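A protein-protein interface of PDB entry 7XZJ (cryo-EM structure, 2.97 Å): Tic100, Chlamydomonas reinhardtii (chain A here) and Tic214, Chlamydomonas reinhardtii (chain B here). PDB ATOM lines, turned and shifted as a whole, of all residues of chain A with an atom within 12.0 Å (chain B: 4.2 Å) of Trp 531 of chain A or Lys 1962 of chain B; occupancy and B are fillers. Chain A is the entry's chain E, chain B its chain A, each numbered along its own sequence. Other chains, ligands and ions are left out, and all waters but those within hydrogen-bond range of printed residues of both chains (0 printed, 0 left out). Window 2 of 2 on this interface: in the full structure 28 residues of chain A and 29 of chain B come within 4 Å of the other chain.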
ATOM      1  N   LYS A 420       5.968  -6.565 -20.799  1.00  0.00           N
ATOM      2  CA  LYS A 420       6.232  -8.027 -20.842  1.00  0.00           C
ATOM      3  C   LYS A 420       6.912  -8.406 -22.160  1.00  0.00           C
ATOM      4  O   LYS A 420       6.768  -7.619 -23.118  1.00  0.00           O
ATOM      5  CB  LYS A 420       4.934  -8.813 -20.633  1.00  0.00           C
ATOM      6  CG  LYS A 420       4.245  -8.577 -19.296  1.00  0.00           C
ATOM      7  CD  LYS A 420       3.132  -9.563 -19.014  1.00  0.00           C
ATOM      8  CE  LYS A 420       3.621 -10.993 -18.922  1.00  0.00           C
ATOM      9  NZ  LYS A 420       2.517 -11.931 -18.612  1.00  0.00           N
ATOM     10  N   ALA A 424      13.019 -11.124 -20.510  1.00  0.00           N
ATOM     11  CA  ALA A 424      13.927 -12.251 -20.829  1.00  0.00           C
ATOM     12  C   ALA A 424      14.471 -12.104 -22.251  1.00  0.00           C
ATOM     13  O   ALA A 424      13.652 -11.905 -23.172  1.00  0.00           O
ATOM     14  CB  ALA A 424      13.197 -13.560 -20.660  1.00  0.00           C
ATOM     15  N   TRP A 531      -2.633 -30.364 -13.006  1.00  0.00           N
ATOM     16  CA  TRP A 531      -2.165 -30.615 -11.617  1.00  0.00           C
ATOM     17  C   TRP A 531      -3.214 -30.096 -10.631  1.00  0.00           C
ATOM     18  O   TRP A 531      -3.252 -28.873 -10.402  1.00  0.00           O
ATOM     19  CB  TRP A 531      -0.805 -29.947 -11.380  1.00  0.00           C
ATOM     20  CG  TRP A 531       0.043 -29.850 -12.611  1.00  0.00           C
ATOM     21  CD1 TRP A 531       0.823 -30.828 -13.154  1.00  0.00           C
ATOM     22  CD2 TRP A 531       0.199 -28.697 -13.457  1.00  0.00           C
ATOM     23  NE1 TRP A 531       1.450 -30.367 -14.280  1.00  0.00           N
ATOM     24  CE2 TRP A 531       1.087 -29.063 -14.491  1.00  0.00           C
ATOM     25  CE3 TRP A 531      -0.324 -27.400 -13.446  1.00  0.00           C
ATOM     26  CZ2 TRP A 531       1.460 -28.176 -15.498  1.00  0.00           C
ATOM     27  CZ3 TRP A 531       0.047 -26.523 -14.440  1.00  0.00           C
ATOM     28  CH2 TRP A 531       0.928 -26.908 -15.451  1.00  0.00           C
ATOM     29  N   GLU A 532      -4.028 -30.995 -10.070  1.00  0.00           N
ATOM     30  CA  GLU A 532      -5.058 -30.587  -9.081  1.00  0.00           C
ATOM     31  C   GLU A 532      -4.343 -29.989  -7.867  1.00  0.00           C
ATOM     32  O   GLU A 532      -4.820 -28.959  -7.355  1.00  0.00           O
ATOM     33  CB  GLU A 532      -5.894 -31.800  -8.673  1.00  0.00           C
ATOM     34  CG  GLU A 532      -6.336 -32.649  -9.849  1.00  0.00           C
ATOM     35  CD  GLU A 532      -6.969 -33.973  -9.458  1.00  0.00           C
ATOM     36  OE1 GLU A 532      -7.082 -34.236  -8.245  1.00  0.00           O
ATOM     37  OE2 GLU A 532      -7.344 -34.738 -10.367  1.00  0.00           O
ATOM     38  N   GLY A 533      -3.242 -30.612  -7.436  1.00  0.00           N
ATOM     39  CA  GLY A 533      -2.451 -30.067  -6.316  1.00  0.00           C
ATOM     40  C   GLY A 533      -1.773 -28.772  -6.717  1.00  0.00           C
ATOM     41  O   GLY A 533      -1.312 -28.687  -7.870  1.00  0.00           O
ATOM     42  N   ALA A 534      -1.693 -27.803  -5.802  1.00  0.00           N
ATOM     43  CA  ALA A 534      -1.127 -26.481  -6.153  1.00  0.00           C
ATOM     44  C   ALA A 534       0.341 -26.383  -5.725  1.00  0.00           C
ATOM     45  O   ALA A 534       0.594 -26.368  -4.503  1.00  0.00           O
ATOM     46  CB  ALA A 534      -1.956 -25.387  -5.523  1.00  0.00           C
ATOM     47  N   THR A 535       1.268 -26.318  -6.686  1.00  0.00           N
ATOM     48  CA  THR A 535       2.704 -26.121  -6.349  1.00  0.00           C
ATOM     49  C   THR A 535       3.183 -24.848  -7.055  1.00  0.00           C
ATOM     50  O   THR A 535       2.951 -24.739  -8.272  1.00  0.00           O
ATOM     51  CB  THR A 535       3.547 -27.331  -6.768  1.00  0.00           C
ATOM     52  OG1 THR A 535       3.237 -27.629  -8.129  1.00  0.00           O
ATOM     53  CG2 THR A 535       3.295 -28.554  -5.912  1.00  0.00           C
ATOM     54  N   ASP A 536       3.819 -23.928  -6.327  1.00  0.00           N
ATOM     55  CA  ASP A 536       4.244 -22.639  -6.934  1.00  0.00           C
ATOM     56  C   ASP A 536       5.480 -22.881  -7.805  1.00  0.00           C
ATOM     57  O   ASP A 536       5.389 -22.667  -9.029  1.00  0.00           O
ATOM     58  CB  ASP A 536       4.503 -21.573  -5.867  1.00  0.00           C
ATOM     59  CG  ASP A 536       3.263 -21.197  -5.077  1.00  0.00           C
ATOM     60  OD1 ASP A 536       2.161 -21.622  -5.479  1.00  0.00           O
ATOM     61  OD2 ASP A 536       3.407 -20.483  -4.065  1.00  0.00           O
ATOM     62  N   SER A 537       6.583 -23.317  -7.192  1.00  0.00           N
ATOM     63  CA  SER A 537       7.840 -23.579  -7.938  1.00  0.00           C
ATOM     64  C   SER A 537       8.505 -24.833  -7.380  1.00  0.00           C
ATOM     65  O   SER A 537       8.462 -25.030  -6.153  1.00  0.00           O
ATOM     66  CB  SER A 537       8.773 -22.416  -7.854  1.00  0.00           C
ATOM     67  OG  SER A 537      10.016 -22.733  -8.462  1.00  0.00           O
ATOM     68  N   GLU A 538       9.122 -25.627  -8.247  1.00  0.00           N
ATOM     69  CA  GLU A 538       9.733 -26.876  -7.823  1.00  0.00           C
ATOM     70  C   GLU A 538      10.978 -26.660  -6.976  1.00  0.00           C
ATOM     71  O   GLU A 538      11.613 -27.639  -6.571  1.00  0.00           O
ATOM     72  CB  GLU A 538      10.077 -27.738  -9.041  1.00  0.00           C
ATOM     73  CG  GLU A 538       9.708 -29.201  -8.885  1.00  0.00           C
ATOM     74  CD  GLU A 538       8.208 -29.426  -8.874  1.00  0.00           C
ATOM     75  OE1 GLU A 538       7.469 -28.548  -9.364  1.00  0.00           O
ATOM     76  OE2 GLU A 538       7.766 -30.481  -8.373  1.00  0.00           O
ATOM     77  N   GLU A 539      11.344 -25.406  -6.705  1.00  0.00           N
ATOM     78  CA  GLU A 539      12.455 -25.136  -5.800  1.00  0.00           C
ATOM     79  C   GLU A 539      12.162 -25.660  -4.398  1.00  0.00           C
ATOM     80  O   GLU A 539      13.084 -26.022  -3.657  1.00  0.00           O
ATOM     81  CB  GLU A 539      12.756 -23.638  -5.770  1.00  0.00           C
ATOM     82  CG  GLU A 539      11.592 -22.757  -5.351  1.00  0.00           C
ATOM     83  CD  GLU A 539      11.669 -22.346  -3.894  1.00  0.00           C
ATOM     84  OE1 GLU A 539      12.661 -22.702  -3.226  1.00  0.00           O
ATOM     85  OE2 GLU A 539      10.737 -21.666  -3.418  1.00  0.00           O
ATOM     86  N   ASN A 540      10.887 -25.685  -4.007  1.00  0.00           N
ATOM     87  CA  ASN A 540      10.480 -26.344  -2.774  1.00  0.00           C
ATOM     88  C   ASN A 540      10.023 -27.756  -3.111  1.00  0.00           C
ATOM     89  O   ASN A 540       8.919 -27.925  -3.653  1.00  0.00           O
ATOM     90  CB  ASN A 540       9.362 -25.570  -2.091  1.00  0.00           C
ATOM     91  CG  ASN A 540       9.870 -24.368  -1.324  1.00  0.00           C
ATOM     92  OD1 ASN A 540      11.059 -24.054  -1.354  1.00  0.00           O
ATOM     93  ND2 ASN A 540       8.967 -23.685  -0.630  1.00  0.00           N
ATOM     94  N   MET A 542       9.120 -32.048  -2.573  1.00  0.00           N
ATOM     95  CA  MET A 542       8.330 -32.871  -1.617  1.00  0.00           C
ATOM     96  C   MET A 542       9.280 -33.726  -0.773  1.00  0.00           C
ATOM     97  O   MET A 542      10.299 -34.193  -1.320  1.00  0.00           O
ATOM     98  CB  MET A 542       7.341 -33.779  -2.355  1.00  0.00           C
ATOM     99  CG  MET A 542       8.002 -34.783  -3.277  1.00  0.00           C
ATOM    100  SD  MET A 542       6.785 -35.711  -4.247  1.00  0.00           S
ATOM    101  CE  MET A 542       5.704 -36.296  -2.944  1.00  0.00           C
ATOM    102  N   LYS B1953      -7.297 -27.235  -8.626  1.00  0.00           N
ATOM    103  CA  LYS B1953      -6.800 -25.832  -8.578  1.00  0.00           C
ATOM    104  C   LYS B1953      -6.013 -25.490  -9.846  1.00  0.00           C
ATOM    105  O   LYS B1953      -5.098 -26.260 -10.193  1.00  0.00           O
ATOM    106  CB  LYS B1953      -5.946 -25.617  -7.324  1.00  0.00           C
ATOM    107  CG  LYS B1953      -5.343 -24.227  -7.168  1.00  0.00           C
ATOM    108  CD  LYS B1953      -6.375 -23.123  -7.071  1.00  0.00           C
ATOM    109  CE  LYS B1953      -7.252 -23.232  -5.843  1.00  0.00           C
ATOM    110  NZ  LYS B1953      -8.269 -22.155  -5.800  1.00  0.00           N
ATOM    111  N   LEU B1955      -3.203 -23.603 -12.102  1.00  0.00           N
ATOM    112  CA  LEU B1955      -1.818 -23.193 -11.746  1.00  0.00           C
ATOM    113  C   LEU B1955      -1.200 -22.396 -12.899  1.00  0.00           C
ATOM    114  O   LEU B1955      -0.127 -22.805 -13.382  1.00  0.00           O
ATOM    115  CB  LEU B1955      -0.991 -24.444 -11.443  1.00  0.00           C
ATOM    116  CG  LEU B1955      -1.095 -24.972 -10.016  1.00  0.00           C
ATOM    117  CD1 LEU B1955      -0.294 -26.254  -9.865  1.00  0.00           C
ATOM    118  CD2 LEU B1955      -0.617 -23.926  -9.022  1.00  0.00           C
ATOM    119  N   LYS B1958       2.229 -21.091 -11.752  1.00  0.00           N
ATOM    120  CA  LYS B1958       3.315 -22.102 -11.856  1.00  0.00           C
ATOM    121  C   LYS B1958       3.791 -22.164 -13.308  1.00  0.00           C
ATOM    122  O   LYS B1958       5.017 -22.209 -13.523  1.00  0.00           O
ATOM    123  CB  LYS B1958       2.795 -23.473 -11.417  1.00  0.00           C
ATOM    124  CG  LYS B1958       3.737 -24.644 -11.663  1.00  0.00           C
ATOM    125  CD  LYS B1958       3.049 -25.989 -11.585  1.00  0.00           C
ATOM    126  CE  LYS B1958       4.006 -27.153 -11.731  1.00  0.00           C
ATOM    127  NZ  LYS B1958       5.034 -27.148 -10.665  1.00  0.00           N
ATOM    128  N   HIS B1959       2.856 -22.131 -14.260  1.00  0.00           N
ATOM    129  CA  HIS B1959       3.213 -22.162 -15.705  1.00  0.00           C
ATOM    130  C   HIS B1959       4.038 -20.919 -16.051  1.00  0.00           C
ATOM    131  O   HIS B1959       4.981 -21.050 -16.847  1.00  0.00           O
ATOM    132  CB  HIS B1959       1.951 -22.317 -16.566  1.00  0.00           C
ATOM    133  CG  HIS B1959       2.213 -22.406 -18.031  1.00  0.00           C
ATOM    134  ND1 HIS B1959       2.955 -23.429 -18.590  1.00  0.00           N
ATOM    135  CD2 HIS B1959       1.827 -21.615 -19.055  1.00  0.00           C
ATOM    136  CE1 HIS B1959       3.024 -23.257 -19.893  1.00  0.00           C
ATOM    137  NE2 HIS B1959       2.339 -22.150 -20.205  1.00  0.00           N
ATOM    138  N   ASN B1960       3.693 -19.765 -15.474  1.00  0.00           N
ATOM    139  CA  ASN B1960       4.405 -18.499 -15.791  1.00  0.00           C
ATOM    140  C   ASN B1960       5.878 -18.609 -15.384  1.00  0.00           C
ATOM    141  O   ASN B1960       6.740 -18.185 -16.174  1.00  0.00           O
ATOM    142  CB  ASN B1960       3.749 -17.301 -15.103  1.00  0.00           C
ATOM    143  CG  ASN B1960       2.406 -16.937 -15.697  1.00  0.00           C
ATOM    144  OD1 ASN B1960       2.110 -17.294 -16.835  1.00  0.00           O
ATOM    145  ND2 ASN B1960       1.594 -16.220 -14.939  1.00  0.00           N
ATOM    146  N   ILE B1961       6.152 -19.173 -14.205  1.00  0.00           N
ATOM    147  CA  ILE B1961       7.564 -19.346 -13.750  1.00  0.00           C
ATOM    148  C   ILE B1961       8.273 -20.287 -14.728  1.00  0.00           C
ATOM    149  O   ILE B1961       9.413 -19.982 -15.125  1.00  0.00           O
ATOM    150  CB  ILE B1961       7.607 -19.881 -12.305  1.00  0.00           C
ATOM    151  CG1 ILE B1961       6.888 -18.943 -11.332  1.00  0.00           C
ATOM    152  CG2 ILE B1961       9.038 -20.150 -11.865  1.00  0.00           C
ATOM    153  CD1 ILE B1961       7.573 -17.612 -11.153  1.00  0.00           C
ATOM    154  N   LYS B1962       7.608 -21.378 -15.117  1.00  0.00           N
ATOM    155  CA  LYS B1962       8.219 -22.367 -16.044  1.00  0.00           C
ATOM    156  C   LYS B1962       8.429 -21.721 -17.419  1.00  0.00           C
ATOM    157  O   LYS B1962       9.467 -22.006 -18.040  1.00  0.00           O
ATOM    158  CB  LYS B1962       7.360 -23.631 -16.123  1.00  0.00           C
ATOM    159  CG  LYS B1962       7.247 -24.409 -14.819  1.00  0.00           C
ATOM    160  CD  LYS B1962       6.530 -25.731 -14.972  1.00  0.00           C
ATOM    161  CE  LYS B1962       5.130 -25.586 -15.528  1.00  0.00           C
ATOM    162  NZ  LYS B1962       4.507 -26.908 -15.774  1.00  0.00           N
ATOM    163  N   VAL B1963       7.480 -20.903 -17.884  1.00  0.00           N
ATOM    164  CA  VAL B1963       7.598 -20.339 -19.263  1.00  0.00           C
ATOM    165  C   VAL B1963       8.810 -19.399 -19.306  1.00  0.00           C
ATOM    166  O   VAL B1963       9.523 -19.410 -20.325  1.00  0.00           O
ATOM    167  CB  VAL B1963       6.286 -19.695 -19.756  1.00  0.00           C
ATOM    168  CG1 VAL B1963       5.858 -18.496 -18.924  1.00  0.00           C
ATOM    169  CG2 VAL B1963       6.361 -19.318 -21.227  1.00  0.00           C
ATOM    170  N   LEU B1964       9.054 -18.655 -18.224  1.00  0.00           N
ATOM    171  CA  LEU B1964      10.241 -17.766 -18.151  1.00  0.00           C
ATOM    172  C   LEU B1964      11.518 -18.604 -18.229  1.00  0.00           C
ATOM    173  O   LEU B1964      12.443 -18.207 -18.966  1.00  0.00           O
ATOM    174  CB  LEU B1964      10.159 -17.015 -16.820  1.00  0.00           C
ATOM    175  CG  LEU B1964      11.135 -15.854 -16.648  1.00  0.00           C
ATOM    176  CD1 LEU B1964      10.952 -14.830 -17.758  1.00  0.00           C
ATOM    177  CD2 LEU B1964      10.953 -15.203 -15.288  1.00  0.00           C
ATOM    178  N   LYS B1965      11.542 -19.740 -17.528  1.00  0.00           N
ATOM    179  CA  LYS B1965      12.757 -20.594 -17.490  1.00  0.00           C
ATOM    180  C   LYS B1965      13.072 -21.087 -18.903  1.00  0.00           C
ATOM    181  O   LYS B1965      14.257 -21.073 -19.280  1.00  0.00           O
ATOM    182  CB  LYS B1965      12.513 -21.781 -16.556  1.00  0.00           C
ATOM    183  CG  LYS B1965      13.733 -22.627 -16.222  1.00  0.00           C
ATOM    184  CD  LYS B1965      13.433 -23.703 -15.202  1.00  0.00           C
ATOM    185  CE  LYS B1965      12.756 -23.165 -13.959  1.00  0.00           C
ATOM    186  NZ  LYS B1965      13.610 -22.185 -13.246  1.00  0.00           N
ATOM    187  N   LYS B1966      12.044 -21.480 -19.658  1.00  0.00           N
ATOM    188  CA  LYS B1966      12.273 -22.035 -21.016  1.00  0.00           C
ATOM    189  C   LYS B1966      12.918 -20.966 -21.901  1.00  0.00           C
ATOM    190  O   LYS B1966      13.885 -21.298 -22.611  1.00  0.00           O
ATOM    191  CB  LYS B1966      10.944 -22.498 -21.619  1.00  0.00           C
ATOM    192  CG  LYS B1966      11.035 -23.120 -23.005  1.00  0.00           C
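Leu 1964 of chain B touches Ala 424 of chain A. Trp 531 of chain A touches Leu 1955 of chain B. CZ2 of Trp 531 of chain A touches NZ of Lys 1962 of chain B (3.3 Å). Gly 533 of chain A touches Leu 1955 of chain B (O to CD1, 3.3 Å). Ala 534 of chain A touches Lys 1953 of chain B (CB to CG, 3.9 Å). Ala 534 of chain A touches Leu 1955 of chain B. Thr 535 of chain A touches Leu 1955 of chain B. O of Asp 536 of chain A touches CA of Lys 1958 of chain B (3.6 Å).
Hydrophobic or aromatic side chains of chain A that line the printed part of chain B: Ala 424, Trp 531 and Ala 534.
Lys 420 of chain A touches none of the printed residues of chain B. Of the printed residues of chain B, Glu 532 of chain A touches Lys 1953. Of the printed residues of chain B, Asp 536 of chain A touches Lys 1958. Met 542 of chain A touches none of the printed residues of chain B. Of the printed residues of chain A, Lys 1953 of chain B touches Trp 531, Glu 532 and Ala 534. Leu 1955 of chain B touches four residues of chain A. No residue of chain A comes within 4 Å of His 1959 of chain B. No residue of chain A comes within 4 Å of Asn 1960 of chain B. No residue of chain A comes within 4 Å of Ile 1961 of chain B. Of chain A, only Trp 531 (3.3 Å) comes within 4 Å of Lys 1962 of chain B. Leu 1964 of chain B touches just one residue of chain A: Ala 424 (3.9 Å). No residue of chain A comes within 4 Å of Lys 1965 of chain B. No residue of chain A comes within 4 Å of Lys 1966 of chain B. The nearest residue of chain B that does not touch Trp 531 of chain A is Lys 1958 of chain B (4.1 Å). The nearest printed residue of chain A that does not touch Lys 1962 of chain B is Asp 536 of chain A (6.3 Å).
The backbone NH (N) of Lys 1953 of chain B sits at hydrogen-bond distance from the backbone carbonyl oxygen (O) of Glu 532 of chain A, at 3.3 Å. OG1 of Thr 535 of chain A is in hydrogen-bond range of NZ of Lys 1958 of chain B (3.1 Å). The side-chain carboxylate of Glu 538 of chain A lies within salt-bridge range of the side-chain amino group of Lys 1958 of chain B. The backbone carbonyl oxygen of Lys 1953 of chain B lies close to the backbone carbonyl oxygen of Trp 531 of chain A (3.2 Å).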
